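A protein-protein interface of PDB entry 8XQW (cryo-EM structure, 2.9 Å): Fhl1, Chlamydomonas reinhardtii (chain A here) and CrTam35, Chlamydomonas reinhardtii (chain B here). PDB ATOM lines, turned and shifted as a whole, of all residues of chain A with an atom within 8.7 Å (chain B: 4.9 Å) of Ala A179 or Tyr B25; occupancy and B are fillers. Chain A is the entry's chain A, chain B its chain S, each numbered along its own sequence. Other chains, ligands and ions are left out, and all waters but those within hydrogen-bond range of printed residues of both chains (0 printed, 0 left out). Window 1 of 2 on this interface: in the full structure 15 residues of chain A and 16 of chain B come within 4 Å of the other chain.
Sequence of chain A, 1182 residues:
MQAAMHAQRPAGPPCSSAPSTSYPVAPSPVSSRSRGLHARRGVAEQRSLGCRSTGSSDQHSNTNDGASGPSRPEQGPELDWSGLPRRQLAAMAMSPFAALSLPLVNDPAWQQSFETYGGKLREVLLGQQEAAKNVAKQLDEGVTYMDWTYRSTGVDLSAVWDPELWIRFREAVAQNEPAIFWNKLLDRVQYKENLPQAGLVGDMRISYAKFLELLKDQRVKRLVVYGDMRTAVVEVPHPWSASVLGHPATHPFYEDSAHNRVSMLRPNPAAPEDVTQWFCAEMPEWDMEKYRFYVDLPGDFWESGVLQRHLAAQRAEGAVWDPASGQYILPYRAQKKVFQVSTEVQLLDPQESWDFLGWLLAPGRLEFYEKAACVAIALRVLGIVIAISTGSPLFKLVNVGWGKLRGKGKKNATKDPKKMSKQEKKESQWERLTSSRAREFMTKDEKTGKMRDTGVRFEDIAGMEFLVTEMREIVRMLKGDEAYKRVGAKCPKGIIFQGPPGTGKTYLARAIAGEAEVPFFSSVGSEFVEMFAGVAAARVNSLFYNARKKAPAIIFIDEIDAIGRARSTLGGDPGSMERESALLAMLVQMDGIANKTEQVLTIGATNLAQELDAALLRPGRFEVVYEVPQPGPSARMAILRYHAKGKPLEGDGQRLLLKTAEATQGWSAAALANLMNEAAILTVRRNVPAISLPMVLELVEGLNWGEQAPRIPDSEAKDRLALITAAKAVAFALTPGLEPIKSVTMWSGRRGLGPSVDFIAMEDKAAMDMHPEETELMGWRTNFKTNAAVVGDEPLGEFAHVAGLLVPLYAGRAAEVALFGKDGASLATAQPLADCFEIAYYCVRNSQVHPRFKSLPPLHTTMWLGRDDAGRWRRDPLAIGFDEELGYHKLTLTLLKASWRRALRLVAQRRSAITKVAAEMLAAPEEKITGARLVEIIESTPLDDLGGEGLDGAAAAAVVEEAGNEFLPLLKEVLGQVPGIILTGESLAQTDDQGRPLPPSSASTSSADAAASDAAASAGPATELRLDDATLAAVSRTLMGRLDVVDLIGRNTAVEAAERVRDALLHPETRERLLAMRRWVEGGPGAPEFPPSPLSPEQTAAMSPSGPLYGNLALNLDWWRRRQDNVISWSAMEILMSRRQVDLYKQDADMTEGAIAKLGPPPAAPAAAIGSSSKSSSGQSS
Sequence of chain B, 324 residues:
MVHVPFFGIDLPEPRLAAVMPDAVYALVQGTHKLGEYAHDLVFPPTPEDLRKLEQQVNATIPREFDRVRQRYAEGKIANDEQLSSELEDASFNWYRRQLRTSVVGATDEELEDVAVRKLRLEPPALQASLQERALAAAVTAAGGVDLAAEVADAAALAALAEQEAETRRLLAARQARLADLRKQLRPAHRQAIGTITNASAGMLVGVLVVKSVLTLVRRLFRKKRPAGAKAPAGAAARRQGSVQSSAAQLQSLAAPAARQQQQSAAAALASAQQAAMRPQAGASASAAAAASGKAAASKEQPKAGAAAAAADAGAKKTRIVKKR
O of Tyr B25 lies close to OE1 of Gln B29.
CD2 of Leu B27 touches CE1 of Phe A169, at 3.96 Å.
Asn A176 touches Gln B29.
CE1 of Tyr B25 touches CB of Pro A178, 3.4 Å away.
CG of Pro A178 touches CG1 of Val B28, 3.99 Å away.
NE2 of Gln B29 touches CG of Pro A178 (3.5 Å).
Ala A179 touches Tyr B25 (N to OH, 3.96 Å).
Val B24 touches Trp A182.
Of chain A, only Pro A178 and Ala A179 come within 4 Å of Tyr B25.
No residue of chain A comes within 4 Å of Ala B26.
Of the printed residues of chain A, Leu B27 touches Phe A169 (3.96 Å).
Of the printed residues of chain A, Val B28 touches Pro A178 (3.99 Å).
Of the printed residues of chain A, Gln B29 touches Asn A176 (3.5 Å) and Pro A178 (3.5 Å).
Asp A187 touches none of the printed residues of chain B.
Ala A172 touches none of the printed residues of chain B.
The nearest printed residue of chain B that does not touch Ala A179 is Val B28 (6.4 Å).
The nearest residue of chain A that does not touch Tyr B25 is Trp A182 (4.4 Å).
The nearest printed residue of chain A that does not touch Val B28 is Ala A172 (4.2 Å).
Of the 10 printed residues of chain B, 5 touch a printed residue of chain A.
Of the 17 printed residues of chain A, 5 touch a printed residue of chain B.
Hydrophobic or aromatic side chains of chain A that line the printed part of chain B: Phe A169, Pro A178 and Trp A182.
Among the printed residues, no Asp or Glu carboxylate lies within 4 Å of a Lys or Arg side-chain nitrogen of the other chain.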
ATOM      1  N   LEU A 165     -23.038  15.331 -18.912  1.00  0.00           N
ATOM      2  CA  LEU A 165     -24.063  16.361 -18.885  1.00  0.00           C
ATOM      3  C   LEU A 165     -25.343  15.856 -18.243  1.00  0.00           C
ATOM      4  O   LEU A 165     -26.011  16.605 -17.526  1.00  0.00           O
ATOM      5  CB  LEU A 165     -24.331  16.867 -20.294  1.00  0.00           C
ATOM      6  CG  LEU A 165     -23.721  18.220 -20.625  1.00  0.00           C
ATOM      7  CD1 LEU A 165     -24.470  18.863 -21.753  1.00  0.00           C
ATOM      8  CD2 LEU A 165     -23.767  19.104 -19.417  1.00  0.00           C
ATOM      9  N   ARG A 168     -24.766  15.767 -14.451  1.00  0.00           N
ATOM     10  CA  ARG A 168     -24.806  17.110 -13.888  1.00  0.00           C
ATOM     11  C   ARG A 168     -26.223  17.652 -13.855  1.00  0.00           C
ATOM     12  O   ARG A 168     -26.602  18.329 -12.899  1.00  0.00           O
ATOM     13  CB  ARG A 168     -23.907  18.044 -14.678  1.00  0.00           C
ATOM     14  CG  ARG A 168     -22.465  17.668 -14.615  1.00  0.00           C
ATOM     15  CD  ARG A 168     -21.964  17.685 -13.203  1.00  0.00           C
ATOM     16  NE  ARG A 168     -20.584  17.229 -13.140  1.00  0.00           N
ATOM     17  CZ  ARG A 168     -20.188  16.161 -12.467  1.00  0.00           C
ATOM     18  NH1 ARG A 168     -18.912  15.815 -12.466  1.00  0.00           N
ATOM     19  NH2 ARG A 168     -21.066  15.439 -11.789  1.00  0.00           N
ATOM     20  N   PHE A 169     -27.022  17.371 -14.881  1.00  0.00           N
ATOM     21  CA  PHE A 169     -28.427  17.759 -14.845  1.00  0.00           C
ATOM     22  C   PHE A 169     -29.136  17.131 -13.656  1.00  0.00           C
ATOM     23  O   PHE A 169     -29.869  17.805 -12.921  1.00  0.00           O
ATOM     24  CB  PHE A 169     -29.106  17.343 -16.142  1.00  0.00           C
ATOM     25  CG  PHE A 169     -30.537  17.736 -16.225  1.00  0.00           C
ATOM     26  CD1 PHE A 169     -30.889  19.039 -16.508  1.00  0.00           C
ATOM     27  CD2 PHE A 169     -31.534  16.809 -16.030  1.00  0.00           C
ATOM     28  CE1 PHE A 169     -32.202  19.407 -16.590  1.00  0.00           C
ATOM     29  CE2 PHE A 169     -32.852  17.178 -16.111  1.00  0.00           C
ATOM     30  CZ  PHE A 169     -33.184  18.476 -16.391  1.00  0.00           C
ATOM     31  N   ALA A 172     -27.984  18.746 -10.426  1.00  0.00           N
ATOM     32  CA  ALA A 172     -28.461  20.115 -10.328  1.00  0.00           C
ATOM     33  C   ALA A 172     -29.914  20.157  -9.898  1.00  0.00           C
ATOM     34  O   ALA A 172     -30.268  20.902  -8.981  1.00  0.00           O
ATOM     35  CB  ALA A 172     -28.279  20.833 -11.661  1.00  0.00           C
ATOM     36  N   VAL A 173     -30.778  19.364 -10.532  1.00  0.00           N
ATOM     37  CA  VAL A 173     -32.171  19.385 -10.098  1.00  0.00           C
ATOM     38  C   VAL A 173     -32.343  18.742  -8.733  1.00  0.00           C
ATOM     39  O   VAL A 173     -33.319  19.043  -8.039  1.00  0.00           O
ATOM     40  CB  VAL A 173     -33.125  18.710 -11.098  1.00  0.00           C
ATOM     41  CG1 VAL A 173     -32.838  19.180 -12.501  1.00  0.00           C
ATOM     42  CG2 VAL A 173     -33.035  17.212 -10.996  1.00  0.00           C
ATOM     43  N   ASN A 176     -31.107  21.760  -6.523  1.00  0.00           N
ATOM     44  CA  ASN A 176     -31.627  23.069  -6.909  1.00  0.00           C
ATOM     45  C   ASN A 176     -30.509  24.106  -6.961  1.00  0.00           C
ATOM     46  O   ASN A 176     -30.505  25.089  -6.220  1.00  0.00           O
ATOM     47  CB  ASN A 176     -32.750  23.521  -5.976  1.00  0.00           C
ATOM     48  CG  ASN A 176     -33.443  24.777  -6.469  1.00  0.00           C
ATOM     49  OD1 ASN A 176     -33.346  25.834  -5.853  1.00  0.00           O
ATOM     50  ND2 ASN A 176     -34.147  24.665  -7.586  1.00  0.00           N
ATOM     51  N   GLU A 177     -29.541  23.871  -7.842  1.00  0.00           N
ATOM     52  CA  GLU A 177     -28.444  24.809  -8.072  1.00  0.00           C
ATOM     53  C   GLU A 177     -28.139  24.826  -9.557  1.00  0.00           C
ATOM     54  O   GLU A 177     -27.317  24.044 -10.046  1.00  0.00           O
ATOM     55  CB  GLU A 177     -27.205  24.435  -7.264  1.00  0.00           C
ATOM     56  CG  GLU A 177     -27.376  24.618  -5.781  1.00  0.00           C
ATOM     57  CD  GLU A 177     -26.057  24.803  -5.079  1.00  0.00           C
ATOM     58  OE1 GLU A 177     -25.013  24.718  -5.757  1.00  0.00           O
ATOM     59  OE2 GLU A 177     -26.063  25.037  -3.853  1.00  0.00           O
ATOM     60  N   PRO A 178     -28.781  25.719 -10.308  1.00  0.00           N
ATOM     61  CA  PRO A 178     -28.635  25.694 -11.769  1.00  0.00           C
ATOM     62  C   PRO A 178     -27.207  25.803 -12.254  1.00  0.00           C
ATOM     63  O   PRO A 178     -26.863  25.152 -13.247  1.00  0.00           O
ATOM     64  CB  PRO A 178     -29.465  26.900 -12.215  1.00  0.00           C
ATOM     65  CG  PRO A 178     -30.455  27.080 -11.137  1.00  0.00           C
ATOM     66  CD  PRO A 178     -29.752  26.730  -9.870  1.00  0.00           C
ATOM     67  N   ALA A 179     -26.365  26.590 -11.580  1.00  0.00           N
ATOM     68  CA  ALA A 179     -24.991  26.776 -12.036  1.00  0.00           C
ATOM     69  C   ALA A 179     -24.310  25.445 -12.297  1.00  0.00           C
ATOM     70  O   ALA A 179     -23.741  25.236 -13.375  1.00  0.00           O
ATOM     71  CB  ALA A 179     -24.202  27.584 -11.011  1.00  0.00           C
ATOM     72  N   ILE A 180     -24.404  24.517 -11.340  1.00  0.00           N
ATOM     73  CA  ILE A 180     -23.770  23.207 -11.459  1.00  0.00           C
ATOM     74  C   ILE A 180     -23.970  22.628 -12.849  1.00  0.00           C
ATOM     75  O   ILE A 180     -23.035  22.096 -13.456  1.00  0.00           O
ATOM     76  CB  ILE A 180     -24.318  22.256 -10.381  1.00  0.00           C
ATOM     77  CG1 ILE A 180     -23.858  22.703  -9.001  1.00  0.00           C
ATOM     78  CG2 ILE A 180     -23.880  20.837 -10.651  1.00  0.00           C
ATOM     79  CD1 ILE A 180     -24.222  21.734  -7.915  1.00  0.00           C
ATOM     80  N   PHE A 181     -25.179  22.737 -13.383  1.00  0.00           N
ATOM     81  CA  PHE A 181     -25.418  22.216 -14.719  1.00  0.00           C
ATOM     82  C   PHE A 181     -24.989  23.215 -15.779  1.00  0.00           C
ATOM     83  O   PHE A 181     -24.203  22.883 -16.669  1.00  0.00           O
ATOM     84  CB  PHE A 181     -26.889  21.860 -14.883  1.00  0.00           C
ATOM     85  CG  PHE A 181     -27.297  21.623 -16.296  1.00  0.00           C
ATOM     86  CD1 PHE A 181     -26.919  20.478 -16.952  1.00  0.00           C
ATOM     87  CD2 PHE A 181     -28.079  22.535 -16.961  1.00  0.00           C
ATOM     88  CE1 PHE A 181     -27.305  20.255 -18.247  1.00  0.00           C
ATOM     89  CE2 PHE A 181     -28.462  22.317 -18.251  1.00  0.00           C
ATOM     90  CZ  PHE A 181     -28.076  21.178 -18.896  1.00  0.00           C
ATOM     91  N   TRP A 182     -25.464  24.454 -15.672  1.00  0.00           N
ATOM     92  CA  TRP A 182     -25.267  25.418 -16.746  1.00  0.00           C
ATOM     93  C   TRP A 182     -23.790  25.650 -17.005  1.00  0.00           C
ATOM     94  O   TRP A 182     -23.345  25.654 -18.155  1.00  0.00           O
ATOM     95  CB  TRP A 182     -25.978  26.719 -16.400  1.00  0.00           C
ATOM     96  CG  TRP A 182     -25.365  27.925 -16.984  1.00  0.00           C
ATOM     97  CD1 TRP A 182     -24.456  28.741 -16.395  1.00  0.00           C
ATOM     98  CD2 TRP A 182     -25.635  28.483 -18.267  1.00  0.00           C
ATOM     99  NE1 TRP A 182     -24.129  29.771 -17.236  1.00  0.00           N
ATOM    100  CE2 TRP A 182     -24.843  29.634 -18.394  1.00  0.00           C
ATOM    101  CE3 TRP A 182     -26.467  28.119 -19.322  1.00  0.00           C
ATOM    102  CZ2 TRP A 182     -24.852  30.419 -19.535  1.00  0.00           C
ATOM    103  CZ3 TRP A 182     -26.475  28.899 -20.452  1.00  0.00           C
ATOM    104  CH2 TRP A 182     -25.676  30.034 -20.552  1.00  0.00           C
ATOM    105  N   ASN A 183     -23.008  25.813 -15.938  1.00  0.00           N
ATOM    106  CA  ASN A 183     -21.570  25.992 -16.090  1.00  0.00           C
ATOM    107  C   ASN A 183     -20.958  24.944 -17.001  1.00  0.00           C
ATOM    108  O   ASN A 183     -20.111  25.276 -17.834  1.00  0.00           O
ATOM    109  CB  ASN A 183     -20.895  25.956 -14.726  1.00  0.00           C
ATOM    110  CG  ASN A 183     -20.777  27.320 -14.109  1.00  0.00           C
ATOM    111  OD1 ASN A 183     -21.022  28.324 -14.764  1.00  0.00           O
ATOM    112  ND2 ASN A 183     -20.397  27.368 -12.843  1.00  0.00           N
ATOM    113  N   LYS A 184     -21.372  23.682 -16.878  1.00  0.00           N
ATOM    114  CA  LYS A 184     -20.844  22.660 -17.775  1.00  0.00           C
ATOM    115  C   LYS A 184     -21.293  22.908 -19.201  1.00  0.00           C
ATOM    116  O   LYS A 184     -20.466  22.963 -20.115  1.00  0.00           O
ATOM    117  CB  LYS A 184     -21.284  21.272 -17.328  1.00  0.00           C
ATOM    118  CG  LYS A 184     -20.656  20.816 -16.045  1.00  0.00           C
ATOM    119  CD  LYS A 184     -19.234  20.389 -16.258  1.00  0.00           C
ATOM    120  CE  LYS A 184     -18.598  20.012 -14.942  1.00  0.00           C
ATOM    121  NZ  LYS A 184     -17.182  19.593 -15.107  1.00  0.00           N
ATOM    122  N   LEU A 185     -22.595  23.084 -19.402  1.00  0.00           N
ATOM    123  CA  LEU A 185     -23.126  23.277 -20.743  1.00  0.00           C
ATOM    124  C   LEU A 185     -22.386  24.390 -21.466  1.00  0.00           C
ATOM    125  O   LEU A 185     -21.937  24.215 -22.603  1.00  0.00           O
ATOM    126  CB  LEU A 185     -24.614  23.585 -20.656  1.00  0.00           C
ATOM    127  CG  LEU A 185     -25.339  23.892 -21.951  1.00  0.00           C
ATOM    128  CD1 LEU A 185     -25.333  22.678 -22.826  1.00  0.00           C
ATOM    129  CD2 LEU A 185     -26.748  24.314 -21.643  1.00  0.00           C
ATOM    130  N   LEU A 186     -22.207  25.526 -20.800  1.00  0.00           N
ATOM    131  CA  LEU A 186     -21.552  26.665 -21.423  1.00  0.00           C
ATOM    132  C   LEU A 186     -20.108  26.381 -21.803  1.00  0.00           C
ATOM    133  O   LEU A 186     -19.628  26.946 -22.788  1.00  0.00           O
ATOM    134  CB  LEU A 186     -21.611  27.861 -20.488  1.00  0.00           C
ATOM    135  CG  LEU A 186     -21.024  29.138 -21.062  1.00  0.00           C
ATOM    136  CD1 LEU A 186     -22.083  29.898 -21.808  1.00  0.00           C
ATOM    137  CD2 LEU A 186     -20.451  29.967 -19.953  1.00  0.00           C
ATOM    138  N   ASP A 187     -19.404  25.525 -21.068  1.00  0.00           N
ATOM    139  CA  ASP A 187     -18.036  25.213 -21.458  1.00  0.00           C
ATOM    140  C   ASP A 187     -17.959  24.453 -22.763  1.00  0.00           C
ATOM    141  O   ASP A 187     -16.889  24.408 -23.370  1.00  0.00           O
ATOM    142  CB  ASP A 187     -17.327  24.395 -20.384  1.00  0.00           C
ATOM    143  CG  ASP A 187     -17.391  25.043 -19.029  1.00  0.00           C
ATOM    144  OD1 ASP A 187     -17.771  26.229 -18.962  1.00  0.00           O
ATOM    145  OD2 ASP A 187     -17.052  24.373 -18.029  1.00  0.00           O
ATOM    146  N   PRO B  21     -29.449  31.899 -20.056  1.00  0.00           N
ATOM    147  CA  PRO B  21     -29.325  31.490 -18.654  1.00  0.00           C
ATOM    148  C   PRO B  21     -30.649  31.488 -17.922  1.00  0.00           C
ATOM    149  O   PRO B  21     -30.886  30.594 -17.106  1.00  0.00           O
ATOM    150  CB  PRO B  21     -28.344  32.515 -18.067  1.00  0.00           C
ATOM    151  CG  PRO B  21     -28.304  33.618 -19.030  1.00  0.00           C
ATOM    152  CD  PRO B  21     -28.557  33.027 -20.362  1.00  0.00           C
ATOM    153  N   ASP B  22     -31.540  32.439 -18.204  1.00  0.00           N
ATOM    154  CA  ASP B  22     -32.837  32.413 -17.539  1.00  0.00           C
ATOM    155  C   ASP B  22     -33.657  31.213 -17.980  1.00  0.00           C
ATOM    156  O   ASP B  22     -34.389  30.629 -17.178  1.00  0.00           O
ATOM    157  CB  ASP B  22     -33.607  33.705 -17.794  1.00  0.00           C
ATOM    158  CG  ASP B  22     -32.785  34.939 -17.505  1.00  0.00           C
ATOM    159  OD1 ASP B  22     -31.975  34.908 -16.556  1.00  0.00           O
ATOM    160  OD2 ASP B  22     -32.943  35.938 -18.235  1.00  0.00           O
ATOM    161  N   ALA B  23     -33.539  30.817 -19.245  1.00  0.00           N
ATOM    162  CA  ALA B  23     -34.267  29.641 -19.706  1.00  0.00           C
ATOM    163  C   ALA B  23     -33.786  28.382 -18.998  1.00  0.00           C
ATOM    164  O   ALA B  23     -34.597  27.581 -18.511  1.00  0.00           O
ATOM    165  CB  ALA B  23     -34.128  29.496 -21.217  1.00  0.00           C
ATOM    166  N   VAL B  24     -32.469  28.193 -18.909  1.00  0.00           N
ATOM    167  CA  VAL B  24     -31.970  26.989 -18.252  1.00  0.00           C
ATOM    168  C   VAL B  24     -32.274  27.033 -16.760  1.00  0.00           C
ATOM    169  O   VAL B  24     -32.549  25.999 -16.137  1.00  0.00           O
ATOM    170  CB  VAL B  24     -30.469  26.797 -18.529  1.00  0.00           C
ATOM    171  CG1 VAL B  24     -30.205  26.827 -20.023  1.00  0.00           C
ATOM    172  CG2 VAL B  24     -29.644  27.835 -17.813  1.00  0.00           C
ATOM    173  N   TYR B  25     -32.264  28.227 -16.165  1.00  0.00           N
ATOM    174  CA  TYR B  25     -32.588  28.342 -14.749  1.00  0.00           C
ATOM    175  C   TYR B  25     -34.045  28.004 -14.498  1.00  0.00           C
ATOM    176  O   TYR B  25     -34.373  27.307 -13.529  1.00  0.00           O
ATOM    177  CB  TYR B  25     -32.274  29.749 -14.260  1.00  0.00           C
ATOM    178  CG  TYR B  25     -30.850  29.919 -13.820  1.00  0.00           C
ATOM    179  CD1 TYR B  25     -29.813  29.411 -14.575  1.00  0.00           C
ATOM    180  CD2 TYR B  25     -30.543  30.585 -12.650  1.00  0.00           C
ATOM    181  CE1 TYR B  25     -28.509  29.563 -14.181  1.00  0.00           C
ATOM    182  CE2 TYR B  25     -29.241  30.742 -12.247  1.00  0.00           C
ATOM    183  CZ  TYR B  25     -28.229  30.226 -13.017  1.00  0.00           C
ATOM    184  OH  TYR B  25     -26.930  30.373 -12.620  1.00  0.00           O
ATOM    185  N   ALA B  26     -34.935  28.499 -15.353  1.00  0.00           N
ATOM    186  CA  ALA B  26     -36.340  28.150 -15.239  1.00  0.00           C
ATOM    187  C   ALA B  26     -36.532  26.650 -15.349  1.00  0.00           C
ATOM    188  O   ALA B  26     -37.267  26.056 -14.558  1.00  0.00           O
ATOM    189  CB  ALA B  26     -37.150  28.878 -16.309  1.00  0.00           C
ATOM    190  N   LEU B  27     -35.866  26.014 -16.315  1.00  0.00           N
ATOM    191  CA  LEU B  27     -36.004  24.569 -16.460  1.00  0.00           C
ATOM    192  C   LEU B  27     -35.550  23.842 -15.199  1.00  0.00           C
ATOM    193  O   LEU B  27     -36.268  22.983 -14.675  1.00  0.00           O
ATOM    194  CB  LEU B  27     -35.218  24.081 -17.673  1.00  0.00           C
ATOM    195  CG  LEU B  27     -34.806  22.609 -17.644  1.00  0.00           C
ATOM    196  CD1 LEU B  27     -36.012  21.695 -17.779  1.00  0.00           C
ATOM    197  CD2 LEU B  27     -33.796  22.326 -18.742  1.00  0.00           C
ATOM    198  N   VAL B  28     -34.365  24.181 -14.692  1.00  0.00           N
ATOM    199  CA  VAL B  28     -33.830  23.490 -13.519  1.00  0.00           C
ATOM    200  C   VAL B  28     -34.754  23.666 -12.321  1.00  0.00           C
ATOM    201  O   VAL B  28     -35.146  22.691 -11.666  1.00  0.00           O
ATOM    202  CB  VAL B  28     -32.409  23.988 -13.205  1.00  0.00           C
ATOM    203  CG1 VAL B  28     -31.954  23.452 -11.870  1.00  0.00           C
ATOM    204  CG2 VAL B  28     -31.450  23.566 -14.289  1.00  0.00           C
ATOM    205  N   GLN B  29     -35.121  24.911 -12.018  1.00  0.00           N
ATOM    206  CA  GLN B  29     -35.928  25.162 -10.830  1.00  0.00           C
ATOM    207  C   GLN B  29     -37.321  24.568 -10.965  1.00  0.00           C
ATOM    208  O   GLN B  29     -37.862  24.019  -9.997  1.00  0.00           O
ATOM    209  CB  GLN B  29     -36.002  26.661 -10.560  1.00  0.00           C
ATOM    210  CG  GLN B  29     -34.777  27.211  -9.869  1.00  0.00           C
ATOM    211  CD  GLN B  29     -34.327  28.523 -10.462  1.00  0.00           C
ATOM    212  OE1 GLN B  29     -35.025  29.117 -11.279  1.00  0.00           O
ATOM    213  NE2 GLN B  29     -33.152  28.980 -10.060  1.00  0.00           N
ATOM    214  N   GLY B  30     -37.922  24.662 -12.151  1.00  0.00           N
ATOM    215  CA  GLY B  30     -39.244  24.097 -12.341  1.00  0.00           C
ATOM    216  C   GLY B  30     -39.249  22.589 -12.219  1.00  0.00           C
ATOM    217  O   GLY B  30     -40.165  22.011 -11.632  1.00  0.00           O
